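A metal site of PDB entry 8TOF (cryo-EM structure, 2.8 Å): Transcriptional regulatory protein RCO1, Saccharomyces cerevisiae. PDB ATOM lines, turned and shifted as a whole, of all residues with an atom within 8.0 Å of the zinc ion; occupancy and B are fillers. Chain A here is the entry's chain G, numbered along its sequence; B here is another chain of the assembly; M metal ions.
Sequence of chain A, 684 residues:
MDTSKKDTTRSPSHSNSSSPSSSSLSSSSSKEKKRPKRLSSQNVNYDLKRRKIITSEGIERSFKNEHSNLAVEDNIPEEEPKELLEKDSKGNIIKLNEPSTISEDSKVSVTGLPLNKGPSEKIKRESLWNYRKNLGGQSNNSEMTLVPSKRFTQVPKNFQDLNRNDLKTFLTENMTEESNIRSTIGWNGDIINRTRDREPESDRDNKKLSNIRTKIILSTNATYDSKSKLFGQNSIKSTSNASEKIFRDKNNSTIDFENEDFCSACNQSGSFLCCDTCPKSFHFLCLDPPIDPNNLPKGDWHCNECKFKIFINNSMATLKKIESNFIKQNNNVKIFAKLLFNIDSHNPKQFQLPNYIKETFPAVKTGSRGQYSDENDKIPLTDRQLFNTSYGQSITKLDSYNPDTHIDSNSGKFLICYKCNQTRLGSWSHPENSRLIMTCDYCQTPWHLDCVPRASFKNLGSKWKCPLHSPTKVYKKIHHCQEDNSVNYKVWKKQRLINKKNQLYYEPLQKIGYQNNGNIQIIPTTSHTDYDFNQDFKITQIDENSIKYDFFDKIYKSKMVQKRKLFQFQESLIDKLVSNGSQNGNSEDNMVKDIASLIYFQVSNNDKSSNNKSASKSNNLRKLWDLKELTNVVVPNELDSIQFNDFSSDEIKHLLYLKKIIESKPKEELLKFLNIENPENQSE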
ATOM      1  N   PHE A 262      -2.145  -4.524  12.013  1.00  0.00           N
ATOM      2  CA  PHE A 262      -1.769  -3.116  12.029  1.00  0.00           C
ATOM      3  C   PHE A 262      -0.293  -2.985  12.378  1.00  0.00           C
ATOM      4  O   PHE A 262       0.234  -3.739  13.203  1.00  0.00           O
ATOM      5  CB  PHE A 262      -2.613  -2.324  13.029  1.00  0.00           C
ATOM      6  CG  PHE A 262      -3.822  -1.676  12.413  1.00  0.00           C
ATOM      7  CD1 PHE A 262      -4.788  -2.443  11.795  1.00  0.00           C
ATOM      8  CD2 PHE A 262      -3.995  -0.303  12.466  1.00  0.00           C
ATOM      9  CE1 PHE A 262      -5.905  -1.863  11.234  1.00  0.00           C
ATOM     10  CE2 PHE A 262      -5.101   0.285  11.909  1.00  0.00           C
ATOM     11  CZ  PHE A 262      -6.063  -0.494  11.287  1.00  0.00           C
ATOM     12  N   CYS A 263       0.368  -2.005  11.765  1.00  0.00           N
ATOM     13  CA  CYS A 263       1.787  -1.808  12.004  1.00  0.00           C
ATOM     14  C   CYS A 263       2.004  -1.371  13.453  1.00  0.00           C
ATOM     15  O   CYS A 263       1.485  -0.336  13.875  1.00  0.00           O
ATOM     16  CB  CYS A 263       2.360  -0.764  11.046  1.00  0.00           C
ATOM     17  SG  CYS A 263       4.015  -0.216  11.490  1.00  0.00           S
ATOM     18  N   SER A 264       2.788  -2.146  14.186  1.00  0.00           N
ATOM     19  CA  SER A 264       2.982  -1.909  15.612  1.00  0.00           C
ATOM     20  C   SER A 264       3.767  -0.641  15.864  1.00  0.00           C
ATOM     21  O   SER A 264       3.836  -0.168  17.001  1.00  0.00           O
ATOM     22  CB  SER A 264       3.680  -3.108  16.250  1.00  0.00           C
ATOM     23  OG  SER A 264       3.152  -4.330  15.777  1.00  0.00           O
ATOM     24  N   ALA A 265       4.365  -0.072  14.818  1.00  0.00           N
ATOM     25  CA  ALA A 265       5.191   1.123  14.942  1.00  0.00           C
ATOM     26  C   ALA A 265       4.412   2.403  14.702  1.00  0.00           C
ATOM     27  O   ALA A 265       4.506   3.345  15.497  1.00  0.00           O
ATOM     28  CB  ALA A 265       6.373   1.041  13.978  1.00  0.00           C
ATOM     29  N   CYS A 266       3.640   2.466  13.618  1.00  0.00           N
ATOM     30  CA  CYS A 266       2.832   3.631  13.309  1.00  0.00           C
ATOM     31  C   CYS A 266       1.335   3.391  13.483  1.00  0.00           C
ATOM     32  O   CYS A 266       0.555   4.337  13.317  1.00  0.00           O
ATOM     33  CB  CYS A 266       3.110   4.110  11.876  1.00  0.00           C
ATOM     34  SG  CYS A 266       2.312   3.142  10.588  1.00  0.00           S
ATOM     35  N   ASN A 267       0.924   2.171  13.824  1.00  0.00           N
ATOM     36  CA  ASN A 267      -0.474   1.859  14.091  1.00  0.00           C
ATOM     37  C   ASN A 267      -1.352   2.201  12.882  1.00  0.00           C
ATOM     38  O   ASN A 267      -2.264   3.022  12.941  1.00  0.00           O
ATOM     39  CB  ASN A 267      -0.971   2.597  15.344  1.00  0.00           C
ATOM     40  CG  ASN A 267      -0.053   2.418  16.525  1.00  0.00           C
ATOM     41  OD1 ASN A 267       0.875   1.598  16.493  1.00  0.00           O
ATOM     42  ND2 ASN A 267      -0.301   3.170  17.593  1.00  0.00           N
ATOM     43  N   GLN A 268      -1.042   1.538  11.768  1.00  0.00           N
ATOM     44  CA  GLN A 268      -1.791   1.720  10.535  1.00  0.00           C
ATOM     45  C   GLN A 268      -1.678   0.435   9.717  1.00  0.00           C
ATOM     46  O   GLN A 268      -1.029  -0.533  10.132  1.00  0.00           O
ATOM     47  CB  GLN A 268      -1.287   2.932   9.760  1.00  0.00           C
ATOM     48  CG  GLN A 268      -1.451   4.250  10.518  1.00  0.00           C
ATOM     49  CD  GLN A 268      -1.121   5.456   9.681  1.00  0.00           C
ATOM     50  OE1 GLN A 268      -1.310   5.458   8.467  1.00  0.00           O
ATOM     51  NE2 GLN A 268      -0.617   6.501  10.330  1.00  0.00           N
ATOM     52  N   SER A 269      -2.333   0.425   8.557  1.00  0.00           N
ATOM     53  CA  SER A 269      -2.450  -0.762   7.733  1.00  0.00           C
ATOM     54  C   SER A 269      -1.524  -0.686   6.530  1.00  0.00           C
ATOM     55  O   SER A 269      -1.095   0.383   6.109  1.00  0.00           O
ATOM     56  CB  SER A 269      -3.892  -0.940   7.268  1.00  0.00           C
ATOM     57  OG  SER A 269      -4.445   0.301   6.862  1.00  0.00           O
ATOM     58  N   GLY A 270      -1.221  -1.859   5.976  1.00  0.00           N
ATOM     59  CA  GLY A 270      -0.369  -1.934   4.810  1.00  0.00           C
ATOM     60  C   GLY A 270       0.310  -3.289   4.734  1.00  0.00           C
ATOM     61  O   GLY A 270       0.015  -4.198   5.516  1.00  0.00           O
ATOM     62  N   SER A 271       1.234  -3.399   3.786  1.00  0.00           N
ATOM     63  CA  SER A 271       2.038  -4.599   3.660  1.00  0.00           C
ATOM     64  C   SER A 271       2.939  -4.743   4.879  1.00  0.00           C
ATOM     65  O   SER A 271       3.443  -3.755   5.416  1.00  0.00           O
ATOM     66  CB  SER A 271       2.868  -4.566   2.380  1.00  0.00           C
ATOM     67  OG  SER A 271       2.200  -5.221   1.322  1.00  0.00           O
ATOM     68  N   PHE A 272       3.138  -5.983   5.304  1.00  0.00           N
ATOM     69  CA  PHE A 272       3.813  -6.243   6.567  1.00  0.00           C
ATOM     70  C   PHE A 272       4.824  -7.367   6.428  1.00  0.00           C
ATOM     71  O   PHE A 272       4.581  -8.346   5.705  1.00  0.00           O
ATOM     72  CB  PHE A 272       2.811  -6.610   7.661  1.00  0.00           C
ATOM     73  CG  PHE A 272       1.803  -5.540   7.941  1.00  0.00           C
ATOM     74  CD1 PHE A 272       2.201  -4.230   8.162  1.00  0.00           C
ATOM     75  CD2 PHE A 272       0.453  -5.840   7.990  1.00  0.00           C
ATOM     76  CE1 PHE A 272       1.272  -3.241   8.422  1.00  0.00           C
ATOM     77  CE2 PHE A 272      -0.479  -4.861   8.252  1.00  0.00           C
ATOM     78  CZ  PHE A 272      -0.067  -3.555   8.473  1.00  0.00           C
ATOM     79  N   SER A 281       3.622  -6.823  14.131  1.00  0.00           N
ATOM     80  CA  SER A 281       3.808  -6.649  12.695  1.00  0.00           C
ATOM     81  C   SER A 281       4.178  -5.202  12.407  1.00  0.00           C
ATOM     82  O   SER A 281       3.706  -4.291  13.095  1.00  0.00           O
ATOM     83  CB  SER A 281       2.549  -7.044  11.930  1.00  0.00           C
ATOM     84  OG  SER A 281       2.576  -6.530  10.615  1.00  0.00           O
ATOM     85  N   PHE A 282       5.003  -5.013  11.386  1.00  0.00           N
ATOM     86  CA  PHE A 282       5.498  -3.683  11.023  1.00  0.00           C
ATOM     87  C   PHE A 282       5.387  -3.482   9.516  1.00  0.00           C
ATOM     88  O   PHE A 282       5.326  -4.439   8.742  1.00  0.00           O
ATOM     89  CB  PHE A 282       6.958  -3.489  11.440  1.00  0.00           C
ATOM     90  CG  PHE A 282       7.194  -3.586  12.907  1.00  0.00           C
ATOM     91  CD1 PHE A 282       7.050  -2.477  13.713  1.00  0.00           C
ATOM     92  CD2 PHE A 282       7.580  -4.785  13.473  1.00  0.00           C
ATOM     93  CE1 PHE A 282       7.265  -2.561  15.071  1.00  0.00           C
ATOM     94  CE2 PHE A 282       7.808  -4.872  14.830  1.00  0.00           C
ATOM     95  CZ  PHE A 282       7.649  -3.762  15.622  1.00  0.00           C
ATOM     96  N   HIS A 283       5.374  -2.217   9.112  1.00  0.00           N
ATOM     97  CA  HIS A 283       5.572  -1.886   7.723  1.00  0.00           C
ATOM     98  C   HIS A 283       7.017  -2.192   7.330  1.00  0.00           C
ATOM     99  O   HIS A 283       7.855  -2.523   8.164  1.00  0.00           O
ATOM    100  CB  HIS A 283       5.255  -0.414   7.466  1.00  0.00           C
ATOM    101  CG  HIS A 283       3.794  -0.096   7.518  1.00  0.00           C
ATOM    102  ND1 HIS A 283       3.289   0.888   8.340  1.00  0.00           N
ATOM    103  CD2 HIS A 283       2.742  -0.631   6.870  1.00  0.00           C
ATOM    104  CE1 HIS A 283       1.976   0.957   8.189  1.00  0.00           C
ATOM    105  NE2 HIS A 283       1.622   0.047   7.296  1.00  0.00           N
ATOM    106  N   PHE A 284       7.298  -2.088   6.037  1.00  0.00           N
ATOM    107  CA  PHE A 284       8.667  -2.249   5.578  1.00  0.00           C
ATOM    108  C   PHE A 284       9.475  -0.967   5.730  1.00  0.00           C
ATOM    109  O   PHE A 284      10.701  -1.031   5.888  1.00  0.00           O
ATOM    110  CB  PHE A 284       8.680  -2.703   4.110  1.00  0.00           C
ATOM    111  CG  PHE A 284       8.091  -4.061   3.902  1.00  0.00           C
ATOM    112  CD1 PHE A 284       6.724  -4.243   3.937  1.00  0.00           C
ATOM    113  CD2 PHE A 284       8.904  -5.146   3.687  1.00  0.00           C
ATOM    114  CE1 PHE A 284       6.173  -5.500   3.755  1.00  0.00           C
ATOM    115  CE2 PHE A 284       8.360  -6.406   3.498  1.00  0.00           C
ATOM    116  CZ  PHE A 284       6.996  -6.578   3.531  1.00  0.00           C
ATOM    117  N   LEU A 285       8.823   0.195   5.697  1.00  0.00           N
ATOM    118  CA  LEU A 285       9.483   1.473   5.879  1.00  0.00           C
ATOM    119  C   LEU A 285       9.371   1.970   7.311  1.00  0.00           C
ATOM    120  O   LEU A 285       9.805   3.095   7.609  1.00  0.00           O
ATOM    121  CB  LEU A 285       8.898   2.497   4.903  1.00  0.00           C
ATOM    122  CG  LEU A 285       9.788   3.708   4.613  1.00  0.00           C
ATOM    123  CD1 LEU A 285      10.810   3.372   3.549  1.00  0.00           C
ATOM    124  CD2 LEU A 285       8.949   4.885   4.174  1.00  0.00           C
ATOM    125  N   CYS A 286       8.794   1.168   8.206  1.00  0.00           N
ATOM    126  CA  CYS A 286       8.727   1.498   9.617  1.00  0.00           C
ATOM    127  C   CYS A 286       9.721   0.720  10.461  1.00  0.00           C
ATOM    128  O   CYS A 286       9.896   1.045  11.646  1.00  0.00           O
ATOM    129  CB  CYS A 286       7.315   1.253  10.161  1.00  0.00           C
ATOM    130  SG  CYS A 286       6.113   2.545   9.762  1.00  0.00           S
ATOM    131  N   LEU A 287      10.394  -0.275   9.901  1.00  0.00           N
ATOM    132  CA  LEU A 287      11.417  -1.014  10.626  1.00  0.00           C
ATOM    133  C   LEU A 287      12.662  -0.147  10.777  1.00  0.00           C
ATOM    134  O   LEU A 287      12.689   1.027  10.394  1.00  0.00           O
ATOM    135  CB  LEU A 287      11.740  -2.324   9.916  1.00  0.00           C
ATOM    136  CG  LEU A 287      10.644  -3.383   9.956  1.00  0.00           C
ATOM    137  CD1 LEU A 287      10.992  -4.534   9.038  1.00  0.00           C
ATOM    138  CD2 LEU A 287      10.413  -3.876  11.380  1.00  0.00           C
ATOM    139  N   PRO A 348      10.941  -0.208  16.795  1.00  0.00           N
ATOM    140  CA  PRO A 348      10.732   1.155  16.289  1.00  0.00           C
ATOM    141  C   PRO A 348       9.314   1.617  16.562  1.00  0.00           C
ATOM    142  O   PRO A 348       8.362   0.830  16.527  1.00  0.00           O
ATOM    143  CB  PRO A 348      11.002   1.023  14.791  1.00  0.00           C
ATOM    144  CG  PRO A 348      11.800  -0.223  14.639  1.00  0.00           C
ATOM    145  CD  PRO A 348      11.313  -1.139  15.708  1.00  0.00           C
ATOM    146  N   GLN A 350       6.619   5.067  15.873  1.00  0.00           N
ATOM    147  CA  GLN A 350       6.371   6.362  15.253  1.00  0.00           C
ATOM    148  C   GLN A 350       6.326   7.449  16.322  1.00  0.00           C
ATOM    149  O   GLN A 350       5.805   7.232  17.421  1.00  0.00           O
ATOM    150  CB  GLN A 350       5.058   6.332  14.478  1.00  0.00           C
ATOM    151  CG  GLN A 350       4.819   7.519  13.582  1.00  0.00           C
ATOM    152  CD  GLN A 350       3.357   7.876  13.475  1.00  0.00           C
ATOM    153  OE1 GLN A 350       2.524   7.024  13.166  1.00  0.00           O
ATOM    154  NE2 GLN A 350       3.024   9.135  13.710  1.00  0.00           N
ATOM    155  N   ARG B 300       5.628   9.055  10.309  1.00  0.00           N
ATOM    156  CA  ARG B 300       5.648   8.080   9.235  1.00  0.00           C
ATOM    157  C   ARG B 300       6.109   8.715   7.927  1.00  0.00           C
ATOM    158  O   ARG B 300       6.789   8.069   7.123  1.00  0.00           O
ATOM    159  CB  ARG B 300       4.283   7.434   9.058  1.00  0.00           C
ATOM    160  CG  ARG B 300       4.299   6.264   8.103  1.00  0.00           C
ATOM    161  CD  ARG B 300       2.911   5.749   7.816  1.00  0.00           C
ATOM    162  NE  ARG B 300       2.952   4.485   7.094  1.00  0.00           N
ATOM    163  CZ  ARG B 300       1.908   3.927   6.493  1.00  0.00           C
ATOM    164  NH1 ARG B 300       0.712   4.492   6.515  1.00  0.00           N
ATOM    165  NH2 ARG B 300       2.078   2.790   5.835  1.00  0.00           N
ATOM    166  N   ARG B 303       9.965   8.931   7.419  1.00  0.00           N
ATOM    167  CA  ARG B 303      10.681   7.667   7.416  1.00  0.00           C
ATOM    168  C   ARG B 303      11.076   7.224   6.019  1.00  0.00           C
ATOM    169  O   ARG B 303      11.640   6.139   5.857  1.00  0.00           O
ATOM    170  CB  ARG B 303       9.854   6.595   8.114  1.00  0.00           C
ATOM    171  CG  ARG B 303       9.888   6.706   9.631  1.00  0.00           C
ATOM    172  CD  ARG B 303      10.121   5.376  10.310  1.00  0.00           C
ATOM    173  NE  ARG B 303      11.457   5.286  10.868  1.00  0.00           N
ATOM    174  CZ  ARG B 303      12.088   4.151  11.137  1.00  0.00           C
ATOM    175  NH1 ARG B 303      11.519   2.986  10.909  1.00  0.00           N
ATOM    176  NH2 ARG B 303      13.312   4.187  11.637  1.00  0.00           N
ATOM    177  N   ALA B 398       5.805   6.792   1.004  1.00  0.00           N
ATOM    178  CA  ALA B 398       5.952   6.971   2.447  1.00  0.00           C
ATOM    179  C   ALA B 398       4.705   6.489   3.189  1.00  0.00           C
ATOM    180  O   ALA B 398       4.814   5.817   4.219  1.00  0.00           O
ATOM    181  CB  ALA B 398       6.230   8.435   2.772  1.00  0.00           C
HETATM  182 ZN    ZN M   1       4.001   1.634  10.093  1.00  0.00          ZN
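NE2 of His 283 sits close to NH2 of Arg 300 of chain B, at 3.1 Å.
A ring nitrogen (NE2) of His 283 lies within hydrogen-bond range of the backbone carbonyl oxygen of Ser 269 (3.0 Å).
The guanidinium group of Arg 300 of chain B lies close to the side-chain sulfur of Cys 266 (3.8 Å).
The backbone carbonyl oxygen (O) of Cys 266 lies close to the side-chain amide oxygen (OE1) of Gln 350, 3.3 Å away.
The side-chain sulfur (SG) of Cys 263 sits close to the backbone NH (N) of Ala 265 (3.3 Å).
The backbone carbonyl oxygen (O) of Cys 263 sits close to the side-chain amide oxygen (OD1) of Asn 267 (3.3 Å).
The backbone NH of Cys 263 lies within hydrogen-bond range of the backbone carbonyl oxygen of Gln 268 (2.6 Å).
O of Cys 286 is in hydrogen-bond range of NH1 of Arg 303 of chain B (2.6 Å).
The zinc ion is bound by ND1 of His 283 (2.0 Å), SG of Cys 266 (2.3 Å), SG of Cys 263 (2.3 Å) and SG of Cys 286 (2.3 Å).
The zinc ion has four donor atoms within binding distance.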
